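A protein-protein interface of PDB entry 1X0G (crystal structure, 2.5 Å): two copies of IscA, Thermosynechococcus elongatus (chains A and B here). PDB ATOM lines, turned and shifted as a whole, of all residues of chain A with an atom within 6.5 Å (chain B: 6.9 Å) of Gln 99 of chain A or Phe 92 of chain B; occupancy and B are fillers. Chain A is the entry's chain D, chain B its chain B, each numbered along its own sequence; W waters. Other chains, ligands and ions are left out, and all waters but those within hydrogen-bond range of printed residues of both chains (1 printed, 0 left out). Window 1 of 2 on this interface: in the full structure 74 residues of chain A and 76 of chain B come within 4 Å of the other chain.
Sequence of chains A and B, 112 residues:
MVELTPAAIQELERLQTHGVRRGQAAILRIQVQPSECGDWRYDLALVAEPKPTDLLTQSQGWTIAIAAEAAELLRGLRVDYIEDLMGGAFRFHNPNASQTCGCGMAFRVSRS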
ATOM      1  N   CYS A  37      12.016   2.106 -16.996  1.00  0.00           N
ATOM      2  CA  CYS A  37      12.236   2.711 -18.288  1.00  0.00           C
ATOM      3  C   CYS A  37      11.751   1.804 -19.337  1.00  0.00           C
ATOM      4  O   CYS A  37      11.310   0.726 -19.041  1.00  0.00           O
ATOM      5  CB  CYS A  37      13.709   2.918 -18.447  1.00  0.00           C
ATOM      6  SG  CYS A  37      14.527   1.399 -18.633  1.00  0.00           S
ATOM      7  N   ASN A  94      21.488  -8.124 -22.754  1.00  0.00           N
ATOM      8  CA  ASN A  94      21.653  -7.526 -24.042  1.00  0.00           C
ATOM      9  C   ASN A  94      22.514  -6.339 -23.813  1.00  0.00           C
ATOM     10  O   ASN A  94      22.089  -5.395 -23.214  1.00  0.00           O
ATOM     11  CB  ASN A  94      20.302  -7.140 -24.672  1.00  0.00           C
ATOM     12  CG  ASN A  94      20.450  -6.643 -26.098  1.00  0.00           C
ATOM     13  OD1 ASN A  94      21.587  -6.466 -26.601  1.00  0.00           O
ATOM     14  ND2 ASN A  94      19.333  -6.439 -26.778  1.00  0.00           N
ATOM     15  N   PRO A  95      23.753  -6.385 -24.251  1.00  0.00           N
ATOM     16  CA  PRO A  95      24.682  -5.280 -23.990  1.00  0.00           C
ATOM     17  C   PRO A  95      24.249  -3.999 -24.680  1.00  0.00           C
ATOM     18  O   PRO A  95      24.465  -2.928 -24.121  1.00  0.00           O
ATOM     19  CB  PRO A  95      26.006  -5.737 -24.598  1.00  0.00           C
ATOM     20  CG  PRO A  95      25.845  -7.148 -24.962  1.00  0.00           C
ATOM     21  CD  PRO A  95      24.352  -7.469 -25.041  1.00  0.00           C
ATOM     22  N   ASN A  96      23.658  -4.107 -25.873  1.00  0.00           N
ATOM     23  CA  ASN A  96      23.168  -2.952 -26.642  1.00  0.00           C
ATOM     24  C   ASN A  96      22.224  -2.067 -25.866  1.00  0.00           C
ATOM     25  O   ASN A  96      22.452  -0.867 -25.656  1.00  0.00           O
ATOM     26  CB  ASN A  96      22.344  -3.473 -27.799  1.00  0.00           C
ATOM     27  CG  ASN A  96      23.187  -4.015 -28.921  1.00  0.00           C
ATOM     28  OD1 ASN A  96      22.647  -4.748 -29.769  1.00  0.00           O
ATOM     29  ND2 ASN A  96      24.507  -3.666 -28.958  1.00  0.00           N
ATOM     30  N   ALA A  97      21.151  -2.714 -25.467  1.00  0.00           N
ATOM     31  CA  ALA A  97      20.075  -2.163 -24.675  1.00  0.00           C
ATOM     32  C   ALA A  97      20.353  -1.941 -23.141  1.00  0.00           C
ATOM     33  O   ALA A  97      19.413  -1.838 -22.325  1.00  0.00           O
ATOM     34  CB  ALA A  97      18.864  -3.095 -24.856  1.00  0.00           C
ATOM     35  N   SER A  98      21.624  -1.902 -22.722  1.00  0.00           N
ATOM     36  CA  SER A  98      21.899  -1.574 -21.319  1.00  0.00           C
ATOM     37  C   SER A  98      22.290  -0.124 -21.215  1.00  0.00           C
ATOM     38  O   SER A  98      23.436   0.150 -20.740  1.00  0.00           O
ATOM     39  CB  SER A  98      23.033  -2.368 -20.728  1.00  0.00           C
ATOM     40  OG  SER A  98      23.259  -1.805 -19.437  1.00  0.00           O
ATOM     41  N   GLN A  99      21.358   0.764 -21.654  1.00  0.00           N
ATOM     42  CA  GLN A  99      21.705   2.124 -22.104  1.00  0.00           C
ATOM     43  C   GLN A  99      20.491   2.995 -21.953  1.00  0.00           C
ATOM     44  O   GLN A  99      19.449   2.782 -22.527  1.00  0.00           O
ATOM     45  CB  GLN A  99      22.304   2.158 -23.527  1.00  0.00           C
ATOM     46  CG  GLN A  99      22.665   3.553 -24.069  1.00  0.00           C
ATOM     47  CD  GLN A  99      23.792   4.357 -23.313  1.00  0.00           C
ATOM     48  OE1 GLN A  99      24.982   3.918 -23.160  1.00  0.00           O
ATOM     49  NE2 GLN A  99      23.418   5.599 -22.916  1.00  0.00           N
ATOM     50  N   THR A 100      20.652   3.940 -21.074  1.00  0.00           N
ATOM     51  CA  THR A 100      19.596   4.774 -20.674  1.00  0.00           C
ATOM     52  C   THR A 100      20.014   6.234 -20.837  1.00  0.00           C
ATOM     53  O   THR A 100      21.105   6.656 -20.492  1.00  0.00           O
ATOM     54  CB  THR A 100      19.101   4.361 -19.256  1.00  0.00           C
ATOM     55  OG1 THR A 100      17.718   4.689 -19.155  1.00  0.00           O
ATOM     56  CG2 THR A 100      19.829   5.131 -18.181  1.00  0.00           C
ATOM     57  N   CYS A 101      19.149   7.007 -21.457  1.00  0.00           N
ATOM     58  CA  CYS A 101      19.501   8.397 -21.715  1.00  0.00           C
ATOM     59  C   CYS A 101      19.007   9.334 -20.537  1.00  0.00           C
ATOM     60  O   CYS A 101      17.911   9.152 -20.005  1.00  0.00           O
ATOM     61  CB  CYS A 101      19.038   8.725 -23.098  1.00  0.00           C
ATOM     62  SG  CYS A 101      19.298  10.449 -23.452  1.00  0.00           S
ATOM     63  N   GLY A 102      19.852  10.259 -20.078  1.00  0.00           N
ATOM     64  CA  GLY A 102      19.564  11.013 -18.841  1.00  0.00           C
ATOM     65  C   GLY A 102      18.671  12.150 -19.238  1.00  0.00           C
ATOM     66  O   GLY A 102      18.269  12.261 -20.385  1.00  0.00           O
ATOM     67  N   CYS A 103      18.364  13.038 -18.312  1.00  0.00           N
ATOM     68  CA  CYS A 103      17.431  14.148 -18.571  1.00  0.00           C
ATOM     69  C   CYS A 103      18.122  15.257 -19.343  1.00  0.00           C
ATOM     70  O   CYS A 103      19.272  15.611 -19.029  1.00  0.00           O
ATOM     71  CB  CYS A 103      17.017  14.725 -17.266  1.00  0.00           C
ATOM     72  SG  CYS A 103      15.590  15.777 -17.491  1.00  0.00           S
ATOM     73  N   TYR B  42      19.716   6.724 -11.450  1.00  0.00           N
ATOM     74  CA  TYR B  42      20.955   7.167 -10.769  1.00  0.00           C
ATOM     75  C   TYR B  42      20.780   8.550 -10.241  1.00  0.00           C
ATOM     76  O   TYR B  42      20.378   9.468 -11.008  1.00  0.00           O
ATOM     77  CB  TYR B  42      22.097   7.151 -11.734  1.00  0.00           C
ATOM     78  CG  TYR B  42      22.162   5.798 -12.452  1.00  0.00           C
ATOM     79  CD1 TYR B  42      21.693   5.646 -13.739  1.00  0.00           C
ATOM     80  CD2 TYR B  42      22.619   4.663 -11.796  1.00  0.00           C
ATOM     81  CE1 TYR B  42      21.716   4.408 -14.355  1.00  0.00           C
ATOM     82  CE2 TYR B  42      22.649   3.454 -12.389  1.00  0.00           C
ATOM     83  CZ  TYR B  42      22.209   3.312 -13.687  1.00  0.00           C
ATOM     84  OH  TYR B  42      22.231   2.023 -14.309  1.00  0.00           O
ATOM     85  N   ASP B  43      21.035   8.709  -8.938  1.00  0.00           N
ATOM     86  CA  ASP B  43      21.145  10.041  -8.353  1.00  0.00           C
ATOM     87  C   ASP B  43      22.603  10.534  -8.224  1.00  0.00           C
ATOM     88  O   ASP B  43      23.306  10.267  -7.236  1.00  0.00           O
ATOM     89  CB  ASP B  43      20.552  10.053  -6.961  1.00  0.00           C
ATOM     90  CG  ASP B  43      19.057   9.911  -6.939  1.00  0.00           C
ATOM     91  OD1 ASP B  43      18.455  10.676  -6.194  1.00  0.00           O
ATOM     92  OD2 ASP B  43      18.462   9.032  -7.575  1.00  0.00           O
ATOM     93  N   LEU B  44      23.037  11.300  -9.188  1.00  0.00           N
ATOM     94  CA  LEU B  44      24.365  11.818  -9.077  1.00  0.00           C
ATOM     95  C   LEU B  44      24.273  13.120  -8.292  1.00  0.00           C
ATOM     96  O   LEU B  44      23.338  13.898  -8.575  1.00  0.00           O
ATOM     97  CB  LEU B  44      24.848  12.096 -10.477  1.00  0.00           C
ATOM     98  CG  LEU B  44      24.998  10.995 -11.555  1.00  0.00           C
ATOM     99  CD1 LEU B  44      26.405  11.004 -12.076  1.00  0.00           C
ATOM    100  CD2 LEU B  44      24.558   9.603 -11.158  1.00  0.00           C
ATOM    101  N   LEU B  77      28.696   0.636 -14.149  1.00  0.00           N
ATOM    102  CA  LEU B  77      28.223   1.937 -14.674  1.00  0.00           C
ATOM    103  C   LEU B  77      29.323   2.781 -15.325  1.00  0.00           C
ATOM    104  O   LEU B  77      30.407   2.969 -14.763  1.00  0.00           O
ATOM    105  CB  LEU B  77      27.520   2.722 -13.585  1.00  0.00           C
ATOM    106  CG  LEU B  77      27.094   4.130 -13.917  1.00  0.00           C
ATOM    107  CD1 LEU B  77      25.941   3.984 -14.869  1.00  0.00           C
ATOM    108  CD2 LEU B  77      26.713   4.921 -12.683  1.00  0.00           C
ATOM    109  N   ARG B  78      29.041   3.177 -16.552  1.00  0.00           N
ATOM    110  CA  ARG B  78      29.778   4.120 -17.285  1.00  0.00           C
ATOM    111  C   ARG B  78      28.827   5.338 -17.619  1.00  0.00           C
ATOM    112  O   ARG B  78      27.712   5.188 -18.197  1.00  0.00           O
ATOM    113  CB  ARG B  78      30.339   3.501 -18.556  1.00  0.00           C
ATOM    114  CG  ARG B  78      30.940   4.614 -19.470  1.00  0.00           C
ATOM    115  CD  ARG B  78      30.776   4.442 -21.001  1.00  0.00           C
ATOM    116  NE  ARG B  78      31.788   3.490 -21.410  1.00  0.00           N
ATOM    117  CZ  ARG B  78      31.556   2.207 -21.729  1.00  0.00           C
ATOM    118  NH1 ARG B  78      30.291   1.744 -21.750  1.00  0.00           N
ATOM    119  NH2 ARG B  78      32.599   1.381 -22.056  1.00  0.00           N
ATOM    120  N   VAL B  79      29.252   6.531 -17.202  1.00  0.00           N
ATOM    121  CA  VAL B  79      28.485   7.747 -17.392  1.00  0.00           C
ATOM    122  C   VAL B  79      29.130   8.550 -18.558  1.00  0.00           C
ATOM    123  O   VAL B  79      30.345   8.811 -18.578  1.00  0.00           O
ATOM    124  CB  VAL B  79      28.518   8.605 -16.140  1.00  0.00           C
ATOM    125  CG1 VAL B  79      27.639   9.813 -16.350  1.00  0.00           C
ATOM    126  CG2 VAL B  79      28.014   7.871 -14.952  1.00  0.00           C
ATOM    127  N   ASP B  80      28.347   8.880 -19.560  1.00  0.00           N
ATOM    128  CA  ASP B  80      28.913   9.535 -20.697  1.00  0.00           C
ATOM    129  C   ASP B  80      28.036  10.763 -20.810  1.00  0.00           C
ATOM    130  O   ASP B  80      27.165  10.984 -19.948  1.00  0.00           O
ATOM    131  CB  ASP B  80      28.756   8.666 -21.917  1.00  0.00           C
ATOM    132  CG  ASP B  80      29.587   9.133 -23.052  1.00  0.00           C
ATOM    133  OD1 ASP B  80      30.373  10.100 -22.843  1.00  0.00           O
ATOM    134  OD2 ASP B  80      29.477   8.532 -24.156  1.00  0.00           O
ATOM    135  N   ILE B  82      26.482  13.214 -24.215  1.00  0.00           N
ATOM    136  CA  ILE B  82      26.490  13.425 -25.626  1.00  0.00           C
ATOM    137  C   ILE B  82      25.591  14.605 -25.979  1.00  0.00           C
ATOM    138  O   ILE B  82      24.476  14.843 -25.409  1.00  0.00           O
ATOM    139  CB  ILE B  82      25.989  12.165 -26.373  1.00  0.00           C
ATOM    140  CG1 ILE B  82      26.994  11.008 -26.242  1.00  0.00           C
ATOM    141  CG2 ILE B  82      25.708  12.453 -27.873  1.00  0.00           C
ATOM    142  CD1 ILE B  82      26.343   9.656 -26.517  1.00  0.00           C
ATOM    143  N   ALA B  89      22.760  15.349 -23.041  1.00  0.00           N
ATOM    144  CA  ALA B  89      22.238  14.557 -21.967  1.00  0.00           C
ATOM    145  C   ALA B  89      23.272  13.599 -21.509  1.00  0.00           C
ATOM    146  O   ALA B  89      24.020  12.986 -22.293  1.00  0.00           O
ATOM    147  CB  ALA B  89      21.032  13.840 -22.418  1.00  0.00           C
ATOM    148  N   PHE B  90      23.272  13.416 -20.205  1.00  0.00           N
ATOM    149  CA  PHE B  90      24.039  12.309 -19.682  1.00  0.00           C
ATOM    150  C   PHE B  90      23.537  10.969 -20.245  1.00  0.00           C
ATOM    151  O   PHE B  90      22.401  10.865 -20.614  1.00  0.00           O
ATOM    152  CB  PHE B  90      24.144  12.389 -18.166  1.00  0.00           C
ATOM    153  CG  PHE B  90      25.193  13.357 -17.727  1.00  0.00           C
ATOM    154  CD1 PHE B  90      24.863  14.601 -17.240  1.00  0.00           C
ATOM    155  CD2 PHE B  90      26.555  13.045 -17.874  1.00  0.00           C
ATOM    156  CE1 PHE B  90      25.833  15.495 -16.856  1.00  0.00           C
ATOM    157  CE2 PHE B  90      27.550  13.957 -17.479  1.00  0.00           C
ATOM    158  CZ  PHE B  90      27.164  15.185 -16.972  1.00  0.00           C
ATOM    159  N   ARG B  91      24.420   9.982 -20.357  1.00  0.00           N
ATOM    160  CA  ARG B  91      24.104   8.707 -20.866  1.00  0.00           C
ATOM    161  C   ARG B  91      24.632   7.671 -19.869  1.00  0.00           C
ATOM    162  O   ARG B  91      25.804   7.707 -19.469  1.00  0.00           O
ATOM    163  CB  ARG B  91      24.787   8.530 -22.194  1.00  0.00           C
ATOM    164  CG  ARG B  91      24.370   9.429 -23.286  1.00  0.00           C
ATOM    165  CD  ARG B  91      22.972   9.310 -23.597  1.00  0.00           C
ATOM    166  NE  ARG B  91      22.656  10.644 -24.043  1.00  0.00           N
ATOM    167  CZ  ARG B  91      22.320  11.011 -25.279  1.00  0.00           C
ATOM    168  NH1 ARG B  91      22.190  10.133 -26.262  1.00  0.00           N
ATOM    169  NH2 ARG B  91      22.139  12.301 -25.524  1.00  0.00           N
ATOM    170  N   PHE B  92      23.765   6.785 -19.447  1.00  0.00           N
ATOM    171  CA  PHE B  92      24.124   5.915 -18.416  1.00  0.00           C
ATOM    172  C   PHE B  92      24.302   4.559 -19.078  1.00  0.00           C
ATOM    173  O   PHE B  92      23.345   4.097 -19.735  1.00  0.00           O
ATOM    174  CB  PHE B  92      23.034   5.918 -17.359  1.00  0.00           C
ATOM    175  CG  PHE B  92      22.931   7.251 -16.641  1.00  0.00           C
ATOM    176  CD1 PHE B  92      22.044   8.190 -17.031  1.00  0.00           C
ATOM    177  CD2 PHE B  92      23.809   7.585 -15.625  1.00  0.00           C
ATOM    178  CE1 PHE B  92      21.974   9.406 -16.387  1.00  0.00           C
ATOM    179  CE2 PHE B  92      23.773   8.812 -14.988  1.00  0.00           C
ATOM    180  CZ  PHE B  92      22.861   9.722 -15.384  1.00  0.00           C
ATOM    181  N   HIS B  93      25.484   3.940 -18.969  1.00  0.00           N
ATOM    182  CA  HIS B  93      25.649   2.539 -19.438  1.00  0.00           C
ATOM    183  C   HIS B  93      26.035   1.596 -18.274  1.00  0.00           C
ATOM    184  O   HIS B  93      26.950   1.875 -17.552  1.00  0.00           O
ATOM    185  CB  HIS B  93      26.614   2.472 -20.652  1.00  0.00           C
ATOM    186  CG  HIS B  93      26.645   1.132 -21.353  1.00  0.00           C
ATOM    187  ND1 HIS B  93      27.512   0.088 -20.985  1.00  0.00           N
ATOM    188  CD2 HIS B  93      25.948   0.669 -22.432  1.00  0.00           C
ATOM    189  CE1 HIS B  93      27.339  -0.943 -21.793  1.00  0.00           C
ATOM    190  NE2 HIS B  93      26.405  -0.618 -22.680  1.00  0.00           N
ATOM    191  N   ASN B  94      25.315   0.503 -18.067  1.00  0.00           N
ATOM    192  CA  ASN B  94      25.599  -0.419 -16.951  1.00  0.00           C
ATOM    193  C   ASN B  94      25.317  -1.863 -17.323  1.00  0.00           C
ATOM    194  O   ASN B  94      24.169  -2.227 -17.464  1.00  0.00           O
ATOM    195  CB  ASN B  94      24.671  -0.082 -15.820  1.00  0.00           C
ATOM    196  CG  ASN B  94      25.136  -0.581 -14.497  1.00  0.00           C
ATOM    197  OD1 ASN B  94      24.591  -0.164 -13.484  1.00  0.00           O
ATOM    198  ND2 ASN B  94      26.160  -1.433 -14.463  1.00  0.00           N
ATOM    199  N   ALA B  97      22.578  -3.772 -14.911  1.00  0.00           N
ATOM    200  CA  ALA B  97      21.190  -3.316 -15.144  1.00  0.00           C
ATOM    201  C   ALA B  97      20.571  -3.908 -16.405  1.00  0.00           C
ATOM    202  O   ALA B  97      19.314  -4.063 -16.507  1.00  0.00           O
ATOM    203  CB  ALA B  97      21.159  -1.830 -15.307  1.00  0.00           C
ATOM    204  N   SER B  98      21.457  -4.195 -17.378  1.00  0.00           N
ATOM    205  CA  SER B  98      21.123  -4.963 -18.621  1.00  0.00           C
ATOM    206  C   SER B  98      20.482  -6.363 -18.452  1.00  0.00           C
ATOM    207  O   SER B  98      20.074  -6.988 -19.452  1.00  0.00           O
ATOM    208  CB  SER B  98      22.359  -5.147 -19.487  1.00  0.00           C
ATOM    209  OG  SER B  98      22.062  -6.072 -20.497  1.00  0.00           O
HETATM  210  O   HOH W   1      21.240  13.943 -17.983  1.00  0.00           O
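The backbone carbonyl oxygen of Phe 90 of chain B is in hydrogen-bond range of the backbone NH of Gly 102 of chain A (2.7 Å).
NE of Arg 91 of chain B sits at hydrogen-bond distance from SG of Cys 101 of chain A (3.4 Å).
The backbone NH (N) of Phe 92 of chain B sits at hydrogen-bond distance from the backbone carbonyl oxygen (O) of Thr 100 of chain A (2.9 Å).
O of Pro 95 of chain A sits at hydrogen-bond distance from NE2 of His 93 of chain B (3.3 Å).
The backbone carbonyl oxygen (O) of Ser 98 of chain A sits at hydrogen-bond distance from the backbone NH (N) of Asn 94 of chain B (3.3 Å).
The side-chain hydroxyl (OG) of Ser 98 of chain B sits at hydrogen-bond distance from the backbone carbonyl oxygen (O) of Asn 94 of chain A.
OD1 of Asn 94 of chain B sits at hydrogen-bond distance from OH of Tyr 42 of chain B (3.3 Å).
N of Leu 77 of chain B sits close to ND2 of Asn 94 of chain B, at 3.3 Å.
The backbone NH of Arg 78 of chain B sits at hydrogen-bond distance from the backbone carbonyl oxygen of His 93 of chain B, at 2.7 Å.
N of Asp 80 of chain B sits at hydrogen-bond distance from O of Arg 91 of chain B.
NH2 of Arg 91 of chain B sits at hydrogen-bond distance from O of Ile 82 of chain B (3.5 Å).
The guanidinium group of Arg 91 of chain B sits at hydrogen-bond distance from the backbone carbonyl oxygen of Ala 89 of chain B (3.2 Å).
Ser 98 of chain A touches His 93 of chain B (O to CD2, 3.1 Å).
Ser 98 of chain A touches Ser 98 of chain B (CB to CB, 3.1 Å).
NE2 of Gln 99 of chain A touches CB of Arg 91 of chain B, at 3.3 Å.
Phe 92 of chain B touches Gln 99 of chain A.
Gln 99 of chain A touches His 93 of chain B.
Arg 91 of chain B touches Thr 100 of chain A.
SG of Cys 101 of chain A touches CB of Ala 89 of chain B, 3.9 Å away.
Cys 101 of chain A touches Phe 90 of chain B.
Ala 89 of chain B touches Gly 102 of chain A.
Phe 92 of chain B touches Gly 102 of chain A.
Gln 99 of chain A touches just these residues of chain B: Arg 91, Phe 92 and His 93.
Of chain A, only Gln 99 (3.5 Å), Thr 100 (2.9 Å) and Gly 102 (3.8 Å) come within 4 Å of Phe 92 of chain B.
Printed residues of chain B within 4 Å of Thr 100 of chain A: Arg 91 and Phe 92.
Of the printed residues of chain A, Asn 94 of chain B touches Ser 98 (2.2 Å).
Printed residues of chain B within 4 Å of Pro 95 of chain A: His 93.
Val 79 of chain B touches none of the printed residues of chain A.
Asn 96 of chain A touches none of the printed residues of chain B.
Of the 11 printed residues of chain A, 7 touch a printed residue of chain B.
Hydrophobic or aromatic side chains of chain B within 4 Å of the printed part of chain A: Ala 89, Phe 92 and His 93.
Among the printed residues, no Asp or Glu carboxylate lies within 4 Å of a Lys or Arg side-chain nitrogen of the other chain.
Asn 94 of chain A touches Ser 98 of chain B, and with the chains exchanged Ser 98 of chain A touches Asn 94 of chain B.
Ser 98 of chain A touches its own counterpart, Ser 98 of chain B.
Of the 16 pairs that touch across the chains among the printed residues, 3 have their exchanged pair printed and touching as well.
Water W1 lies within hydrogen-bond range of O of Cys 103 of chain A (2.8 Å) and N of Phe 90 of chain B (3.1 Å).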
